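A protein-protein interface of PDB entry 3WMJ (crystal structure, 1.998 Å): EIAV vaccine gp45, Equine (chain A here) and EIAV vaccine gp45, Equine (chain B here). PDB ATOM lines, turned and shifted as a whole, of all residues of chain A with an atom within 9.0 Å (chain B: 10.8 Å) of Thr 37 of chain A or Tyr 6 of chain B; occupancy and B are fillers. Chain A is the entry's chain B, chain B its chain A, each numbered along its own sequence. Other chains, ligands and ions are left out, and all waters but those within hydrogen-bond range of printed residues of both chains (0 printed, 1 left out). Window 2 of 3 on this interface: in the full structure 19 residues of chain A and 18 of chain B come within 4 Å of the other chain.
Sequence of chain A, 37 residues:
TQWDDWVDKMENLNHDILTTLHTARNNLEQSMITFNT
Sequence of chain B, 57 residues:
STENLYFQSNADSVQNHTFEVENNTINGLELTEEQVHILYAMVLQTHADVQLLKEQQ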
ATOM      1  N   GLN A  30     -28.119  -2.321  17.438  1.00  0.00           N
ATOM      2  CA  GLN A  30     -28.011  -2.096  18.885  1.00  0.00           C
ATOM      3  C   GLN A  30     -26.918  -2.949  19.548  1.00  0.00           C
ATOM      4  O   GLN A  30     -26.131  -2.450  20.366  1.00  0.00           O
ATOM      5  CB  GLN A  30     -29.353  -2.355  19.588  1.00  0.00           C
ATOM      6  CG  GLN A  30     -30.512  -1.449  19.143  1.00  0.00           C
ATOM      7  CD  GLN A  30     -31.789  -1.661  19.956  1.00  0.00           C
ATOM      8  OE1 GLN A  30     -32.700  -2.382  19.532  1.00  0.00           O
ATOM      9  NE2 GLN A  30     -31.866  -1.019  21.125  1.00  0.00           N
ATOM     10  N   SER A  31     -26.875  -4.236  19.216  1.00  0.00           N
ATOM     11  CA  SER A  31     -25.914  -5.139  19.872  1.00  0.00           C
ATOM     12  C   SER A  31     -24.483  -4.791  19.487  1.00  0.00           C
ATOM     13  O   SER A  31     -23.559  -4.942  20.300  1.00  0.00           O
ATOM     14  CB  SER A  31     -26.203  -6.620  19.567  1.00  0.00           C
ATOM     15  OG  SER A  31     -26.081  -6.891  18.180  1.00  0.00           O
ATOM     16  N   MET A  32     -24.292  -4.335  18.253  1.00  0.00           N
ATOM     17  CA  MET A  32     -22.951  -3.976  17.814  1.00  0.00           C
ATOM     18  C   MET A  32     -22.501  -2.706  18.531  1.00  0.00           C
ATOM     19  O   MET A  32     -21.383  -2.623  19.046  1.00  0.00           O
ATOM     20  CB  MET A  32     -22.929  -3.800  16.295  1.00  0.00           C
ATOM     21  CG  MET A  32     -23.196  -5.099  15.542  1.00  0.00           C
ATOM     22  SD  MET A  32     -23.243  -4.907  13.740  1.00  0.00           S
ATOM     23  CE  MET A  32     -21.514  -4.546  13.422  1.00  0.00           C
ATOM     24  N   ILE A  33     -23.392  -1.727  18.592  1.00  0.00           N
ATOM     25  CA  ILE A  33     -23.064  -0.459  19.237  1.00  0.00           C
ATOM     26  C   ILE A  33     -22.765  -0.664  20.715  1.00  0.00           C
ATOM     27  O   ILE A  33     -21.756  -0.180  21.228  1.00  0.00           O
ATOM     28  CB  ILE A  33     -24.183   0.575  19.018  1.00  0.00           C
ATOM     29  CG1 ILE A  33     -24.113   1.081  17.576  1.00  0.00           C
ATOM     30  CG2 ILE A  33     -24.067   1.729  20.021  1.00  0.00           C
ATOM     31  CD1 ILE A  33     -25.257   1.935  17.162  1.00  0.00           C
ATOM     32  N   THR A  34     -23.632  -1.405  21.391  1.00  0.00           N
ATOM     33  CA  THR A  34     -23.402  -1.744  22.787  1.00  0.00           C
ATOM     34  C   THR A  34     -22.072  -2.473  22.967  1.00  0.00           C
ATOM     35  O   THR A  34     -21.290  -2.136  23.867  1.00  0.00           O
ATOM     36  CB  THR A  34     -24.540  -2.584  23.341  1.00  0.00           C
ATOM     37  OG1 THR A  34     -25.749  -1.819  23.277  1.00  0.00           O
ATOM     38  CG2 THR A  34     -24.263  -2.956  24.802  1.00  0.00           C
ATOM     39  N   PHE A  35     -21.799  -3.449  22.101  1.00  0.00           N
ATOM     40  CA  PHE A  35     -20.555  -4.213  22.198  1.00  0.00           C
ATOM     41  C   PHE A  35     -19.331  -3.331  21.982  1.00  0.00           C
ATOM     42  O   PHE A  35     -18.269  -3.568  22.574  1.00  0.00           O
ATOM     43  CB  PHE A  35     -20.511  -5.351  21.170  1.00  0.00           C
ATOM     44  CG  PHE A  35     -19.219  -6.138  21.215  1.00  0.00           C
ATOM     45  CD1 PHE A  35     -18.893  -6.889  22.341  1.00  0.00           C
ATOM     46  CD2 PHE A  35     -18.322  -6.098  20.153  1.00  0.00           C
ATOM     47  CE1 PHE A  35     -17.700  -7.615  22.399  1.00  0.00           C
ATOM     48  CE2 PHE A  35     -17.125  -6.822  20.198  1.00  0.00           C
ATOM     49  CZ  PHE A  35     -16.818  -7.583  21.324  1.00  0.00           C
ATOM     50  N   ASN A  36     -19.468  -2.327  21.121  1.00  0.00           N
ATOM     51  CA  ASN A  36     -18.359  -1.409  20.879  1.00  0.00           C
ATOM     52  C   ASN A  36     -18.342  -0.161  21.792  1.00  0.00           C
ATOM     53  O   ASN A  36     -17.693   0.843  21.476  1.00  0.00           O
ATOM     54  CB  ASN A  36     -18.267  -1.058  19.391  1.00  0.00           C
ATOM     55  CG  ASN A  36     -17.759  -2.234  18.554  1.00  0.00           C
ATOM     56  OD1 ASN A  36     -16.562  -2.535  18.547  1.00  0.00           O
ATOM     57  ND2 ASN A  36     -18.669  -2.912  17.868  1.00  0.00           N
ATOM     58  N   THR A  37     -19.039  -0.253  22.926  1.00  0.00           N
ATOM     59  CA  THR A  37     -19.046   0.798  23.954  1.00  0.00           C
ATOM     60  C   THR A  37     -17.707   0.870  24.686  1.00  0.00           C
ATOM     61  O   THR A  37     -17.172   1.956  24.923  1.00  0.00           O
ATOM     62  CB  THR A  37     -20.169   0.574  25.008  1.00  0.00           C
ATOM     63  OG1 THR A  37     -21.448   0.865  24.434  1.00  0.00           O
ATOM     64  CG2 THR A  37     -19.968   1.472  26.227  1.00  0.00           C
ATOM     65  N   SER B   1     -18.612  -0.395  42.628  1.00  0.00           N
ATOM     66  CA  SER B   1     -18.466  -1.405  41.580  1.00  0.00           C
ATOM     67  C   SER B   1     -19.055  -0.924  40.250  1.00  0.00           C
ATOM     68  O   SER B   1     -19.340  -1.736  39.364  1.00  0.00           O
ATOM     69  CB  SER B   1     -19.120  -2.723  42.014  1.00  0.00           C
ATOM     70  N   THR B   2     -19.212   0.395  40.116  1.00  0.00           N
ATOM     71  CA  THR B   2     -19.900   1.022  38.972  1.00  0.00           C
ATOM     72  C   THR B   2     -19.439   0.579  37.573  1.00  0.00           C
ATOM     73  O   THR B   2     -20.267   0.160  36.747  1.00  0.00           O
ATOM     74  CB  THR B   2     -19.808   2.559  39.054  1.00  0.00           C
ATOM     75  OG1 THR B   2     -20.377   3.001  40.289  1.00  0.00           O
ATOM     76  CG2 THR B   2     -20.557   3.195  37.909  1.00  0.00           C
ATOM     77  N   GLU B   3     -18.134   0.688  37.317  1.00  0.00           N
ATOM     78  CA  GLU B   3     -17.531   0.305  36.034  1.00  0.00           C
ATOM     79  C   GLU B   3     -17.906  -1.118  35.645  1.00  0.00           C
ATOM     80  O   GLU B   3     -18.525  -1.351  34.601  1.00  0.00           O
ATOM     81  CB  GLU B   3     -16.001   0.396  36.119  1.00  0.00           C
ATOM     82  CG  GLU B   3     -15.363   1.628  35.476  1.00  0.00           C
ATOM     83  CD  GLU B   3     -15.322   1.541  33.963  1.00  0.00           C
ATOM     84  OE1 GLU B   3     -16.389   1.711  33.330  1.00  0.00           O
ATOM     85  OE2 GLU B   3     -14.223   1.301  33.407  1.00  0.00           O
ATOM     86  N   ASN B   4     -17.500  -2.057  36.492  1.00  0.00           N
ATOM     87  CA  ASN B   4     -17.780  -3.479  36.313  1.00  0.00           C
ATOM     88  C   ASN B   4     -19.276  -3.772  36.154  1.00  0.00           C
ATOM     89  O   ASN B   4     -19.677  -4.531  35.265  1.00  0.00           O
ATOM     90  CB  ASN B   4     -17.171  -4.261  37.493  1.00  0.00           C
ATOM     91  CG  ASN B   4     -17.746  -5.672  37.652  1.00  0.00           C
ATOM     92  OD1 ASN B   4     -18.103  -6.346  36.677  1.00  0.00           O
ATOM     93  ND2 ASN B   4     -17.822  -6.127  38.902  1.00  0.00           N
ATOM     94  N   LEU B   5     -20.095  -3.173  37.016  1.00  0.00           N
ATOM     95  CA  LEU B   5     -21.540  -3.341  36.928  1.00  0.00           C
ATOM     96  C   LEU B   5     -22.076  -2.858  35.576  1.00  0.00           C
ATOM     97  O   LEU B   5     -22.958  -3.497  34.978  1.00  0.00           O
ATOM     98  CB  LEU B   5     -22.239  -2.599  38.070  1.00  0.00           C
ATOM     99  CG  LEU B   5     -22.603  -3.460  39.279  1.00  0.00           C
ATOM    100  CD1 LEU B   5     -23.503  -2.687  40.237  1.00  0.00           C
ATOM    101  CD2 LEU B   5     -23.280  -4.742  38.799  1.00  0.00           C
ATOM    102  N   TYR B   6     -21.535  -1.737  35.098  1.00  0.00           N
ATOM    103  CA  TYR B   6     -21.950  -1.167  33.819  1.00  0.00           C
ATOM    104  C   TYR B   6     -21.590  -2.092  32.657  1.00  0.00           C
ATOM    105  O   TYR B   6     -22.398  -2.322  31.750  1.00  0.00           O
ATOM    106  CB  TYR B   6     -21.317   0.215  33.594  1.00  0.00           C
ATOM    107  CG  TYR B   6     -21.646   0.772  32.228  1.00  0.00           C
ATOM    108  CD1 TYR B   6     -22.966   0.877  31.811  1.00  0.00           C
ATOM    109  CD2 TYR B   6     -20.644   1.171  31.355  1.00  0.00           C
ATOM    110  CE1 TYR B   6     -23.288   1.368  30.560  1.00  0.00           C
ATOM    111  CE2 TYR B   6     -20.952   1.669  30.099  1.00  0.00           C
ATOM    112  CZ  TYR B   6     -22.277   1.761  29.709  1.00  0.00           C
ATOM    113  OH  TYR B   6     -22.600   2.246  28.467  1.00  0.00           O
ATOM    114  N   PHE B   7     -20.373  -2.620  32.686  1.00  0.00           N
ATOM    115  CA  PHE B   7     -19.900  -3.439  31.584  1.00  0.00           C
ATOM    116  C   PHE B   7     -20.509  -4.836  31.582  1.00  0.00           C
ATOM    117  O   PHE B   7     -20.656  -5.459  30.527  1.00  0.00           O
ATOM    118  CB  PHE B   7     -18.379  -3.460  31.569  1.00  0.00           C
ATOM    119  CG  PHE B   7     -17.789  -2.163  31.115  1.00  0.00           C
ATOM    120  CD1 PHE B   7     -18.467  -1.381  30.186  1.00  0.00           C
ATOM    121  CD2 PHE B   7     -16.580  -1.711  31.622  1.00  0.00           C
ATOM    122  CE1 PHE B   7     -17.940  -0.177  29.751  1.00  0.00           C
ATOM    123  CE2 PHE B   7     -16.046  -0.504  31.197  1.00  0.00           C
ATOM    124  CZ  PHE B   7     -16.729   0.266  30.261  1.00  0.00           C
ATOM    125  N   GLN B   8     -20.885  -5.311  32.764  1.00  0.00           N
ATOM    126  CA  GLN B   8     -21.665  -6.535  32.873  1.00  0.00           C
ATOM    127  C   GLN B   8     -23.066  -6.299  32.312  1.00  0.00           C
ATOM    128  O   GLN B   8     -23.645  -7.180  31.671  1.00  0.00           O
ATOM    129  CB  GLN B   8     -21.736  -6.981  34.330  1.00  0.00           C
ATOM    130  CG  GLN B   8     -22.924  -7.868  34.683  1.00  0.00           C
ATOM    131  CD  GLN B   8     -23.025  -8.097  36.184  1.00  0.00           C
ATOM    132  OE1 GLN B   8     -22.065  -8.544  36.820  1.00  0.00           O
ATOM    133  NE2 GLN B   8     -24.180  -7.770  36.760  1.00  0.00           N
ATOM    134  N   SER B   9     -23.600  -5.104  32.551  1.00  0.00           N
ATOM    135  CA  SER B   9     -24.896  -4.726  32.013  1.00  0.00           C
ATOM    136  C   SER B   9     -24.844  -4.689  30.481  1.00  0.00           C
ATOM    137  O   SER B   9     -25.756  -5.176  29.809  1.00  0.00           O
ATOM    138  CB  SER B   9     -25.339  -3.374  32.570  1.00  0.00           C
ATOM    139  OG  SER B   9     -26.587  -2.993  32.005  1.00  0.00           O
ATOM    140  N   ASN B  10     -23.771  -4.120  29.937  1.00  0.00           N
ATOM    141  CA  ASN B  10     -23.568  -4.110  28.491  1.00  0.00           C
ATOM    142  C   ASN B  10     -23.455  -5.513  27.897  1.00  0.00           C
ATOM    143  O   ASN B  10     -24.063  -5.802  26.863  1.00  0.00           O
ATOM    144  CB  ASN B  10     -22.337  -3.288  28.121  1.00  0.00           C
ATOM    145  CG  ASN B  10     -22.577  -1.800  28.248  1.00  0.00           C
ATOM    146  OD1 ASN B  10     -23.725  -1.343  28.320  1.00  0.00           O
ATOM    147  ND2 ASN B  10     -21.497  -1.031  28.264  1.00  0.00           N
ATOM    148  N   ALA B  11     -22.680  -6.375  28.551  1.00  0.00           N
ATOM    149  CA  ALA B  11     -22.539  -7.760  28.105  1.00  0.00           C
ATOM    150  C   ALA B  11     -23.896  -8.465  28.068  1.00  0.00           C
ATOM    151  O   ALA B  11     -24.213  -9.161  27.095  1.00  0.00           O
ATOM    152  CB  ALA B  11     -21.581  -8.515  29.003  1.00  0.00           C
ATOM    153  N   ASP B  12     -24.685  -8.298  29.131  1.00  0.00           N
ATOM    154  CA  ASP B  12     -26.031  -8.855  29.153  1.00  0.00           C
ATOM    155  C   ASP B  12     -26.887  -8.269  28.034  1.00  0.00           C
ATOM    156  O   ASP B  12     -27.675  -8.988  27.403  1.00  0.00           O
ATOM    157  CB  ASP B  12     -26.695  -8.622  30.509  1.00  0.00           C
ATOM    158  CG  ASP B  12     -25.996  -9.367  31.634  1.00  0.00           C
ATOM    159  OD1 ASP B  12     -25.130 -10.225  31.328  1.00  0.00           O
ATOM    160  OD2 ASP B  12     -26.315  -9.096  32.816  1.00  0.00           O
ATOM    161  N   SER B  13     -26.739  -6.967  27.790  1.00  0.00           N
ATOM    162  CA  SER B  13     -27.529  -6.310  26.747  1.00  0.00           C
ATOM    163  C   SER B  13     -27.194  -6.866  25.363  1.00  0.00           C
ATOM    164  O   SER B  13     -28.102  -7.119  24.551  1.00  0.00           O
ATOM    165  CB  SER B  13     -27.326  -4.793  26.770  1.00  0.00           C
ATOM    166  OG  SER B  13     -28.178  -4.180  25.817  1.00  0.00           O
ATOM    167  N   VAL B  14     -25.900  -7.062  25.100  1.00  0.00           N
ATOM    168  CA  VAL B  14     -25.460  -7.645  23.830  1.00  0.00           C
ATOM    169  C   VAL B  14     -26.056  -9.044  23.688  1.00  0.00           C
ATOM    170  O   VAL B  14     -26.631  -9.379  22.646  1.00  0.00           O
ATOM    171  CB  VAL B  14     -23.915  -7.738  23.724  1.00  0.00           C
ATOM    172  CG1 VAL B  14     -23.517  -8.499  22.472  1.00  0.00           C
ATOM    173  CG2 VAL B  14     -23.260  -6.340  23.694  1.00  0.00           C
ATOM    174  N   HIS B  17     -29.877  -8.815  22.975  1.00  0.00           N
ATOM    175  CA  HIS B  17     -30.229  -8.363  21.630  1.00  0.00           C
ATOM    176  C   HIS B  17     -29.911  -9.440  20.589  1.00  0.00           C
ATOM    177  O   HIS B  17     -30.575  -9.533  19.555  1.00  0.00           O
ATOM    178  CB  HIS B  17     -29.564  -7.029  21.319  1.00  0.00           C
ATOM    179  CG  HIS B  17     -30.258  -5.861  21.953  1.00  0.00           C
ATOM    180  ND1 HIS B  17     -29.646  -5.042  22.875  1.00  0.00           N
ATOM    181  CD2 HIS B  17     -31.516  -5.380  21.803  1.00  0.00           C
ATOM    182  CE1 HIS B  17     -30.498  -4.105  23.267  1.00  0.00           C
ATOM    183  NE2 HIS B  17     -31.639  -4.291  22.627  1.00  0.00           N
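The side-chain hydroxyl of Tyr 6 of chain B sits close to the side-chain amide nitrogen of Asn 10 of chain B, at 3.5 Å. O of Ser 13 of chain B lies within hydrogen-bond range of ND1 of His 17 of chain B. The side-chain hydroxyl (OG1) of Thr 34 of chain A is in hydrogen-bond range of the backbone carbonyl oxygen (O) of Gln 30 of chain A, at 3.0 Å. The side-chain hydroxyl (OG1) of Thr 37 of chain A sits at hydrogen-bond distance from the backbone carbonyl oxygen (O) of Ile 33 of chain A (3.4 Å). The backbone carbonyl oxygen (O) of Thr 34 of chain A lies within hydrogen-bond range of the side-chain hydroxyl (OG1) of Thr 37 of chain A (3.1 Å).
Among the printed residues, pairs that only touch across the chains: Thr 34 of chain A with Asn 10 of chain B (3.5 Å), Thr 37 of chain A with Tyr 6 of chain B (3.5 Å), Thr 37 of chain A with Asn 10 of chain B (3.6 Å), Gln 30 of chain A with His 17 of chain B (3.6 Å), Phe 35 of chain A with Val 14 of chain B (3.6 Å), Ser 31 of chain A with Val 14 of chain B (3.7 Å), Thr 34 of chain A with Val 14 of chain B (3.7 Å) and Ser 31 of chain A with His 17 of chain B (3.8 Å).
Thr 34 of chain A touches just these residues of chain B: Asn 10 (3.5 Å) and Val 14 (3.7 Å). Thr 37 of chain A touches just these residues of chain B: Tyr 6 and Asn 10. Ser 1 of chain B touches none of the printed residues of chain A. Of the printed residues of chain A, Tyr 6 of chain B touches Thr 37. Printed residues of chain A within 4 Å of Val 14 of chain B: Ser 31 (3.7 Å), Thr 34 (3.7 Å) and Phe 35 (3.6 Å). Of the printed residues of chain A, His 17 of chain B touches Gln 30 and Ser 31. The nearest residue of chain B that does not touch Thr 37 of chain A is Phe 7 of chain B (4.4 Å). The nearest printed residue of chain B that does not touch Gln 30 of chain A is Val 14 of chain B (5.9 Å).
Of the 15 printed residues of chain B, 4 touch a printed residue of chain A. Printed residues of chain B that touch a printed residue of chain A: Tyr 6, Asn 10, Val 14 and His 17. Along chain A the printed residues that touch a printed residue of chain B span positions 30 to 37.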
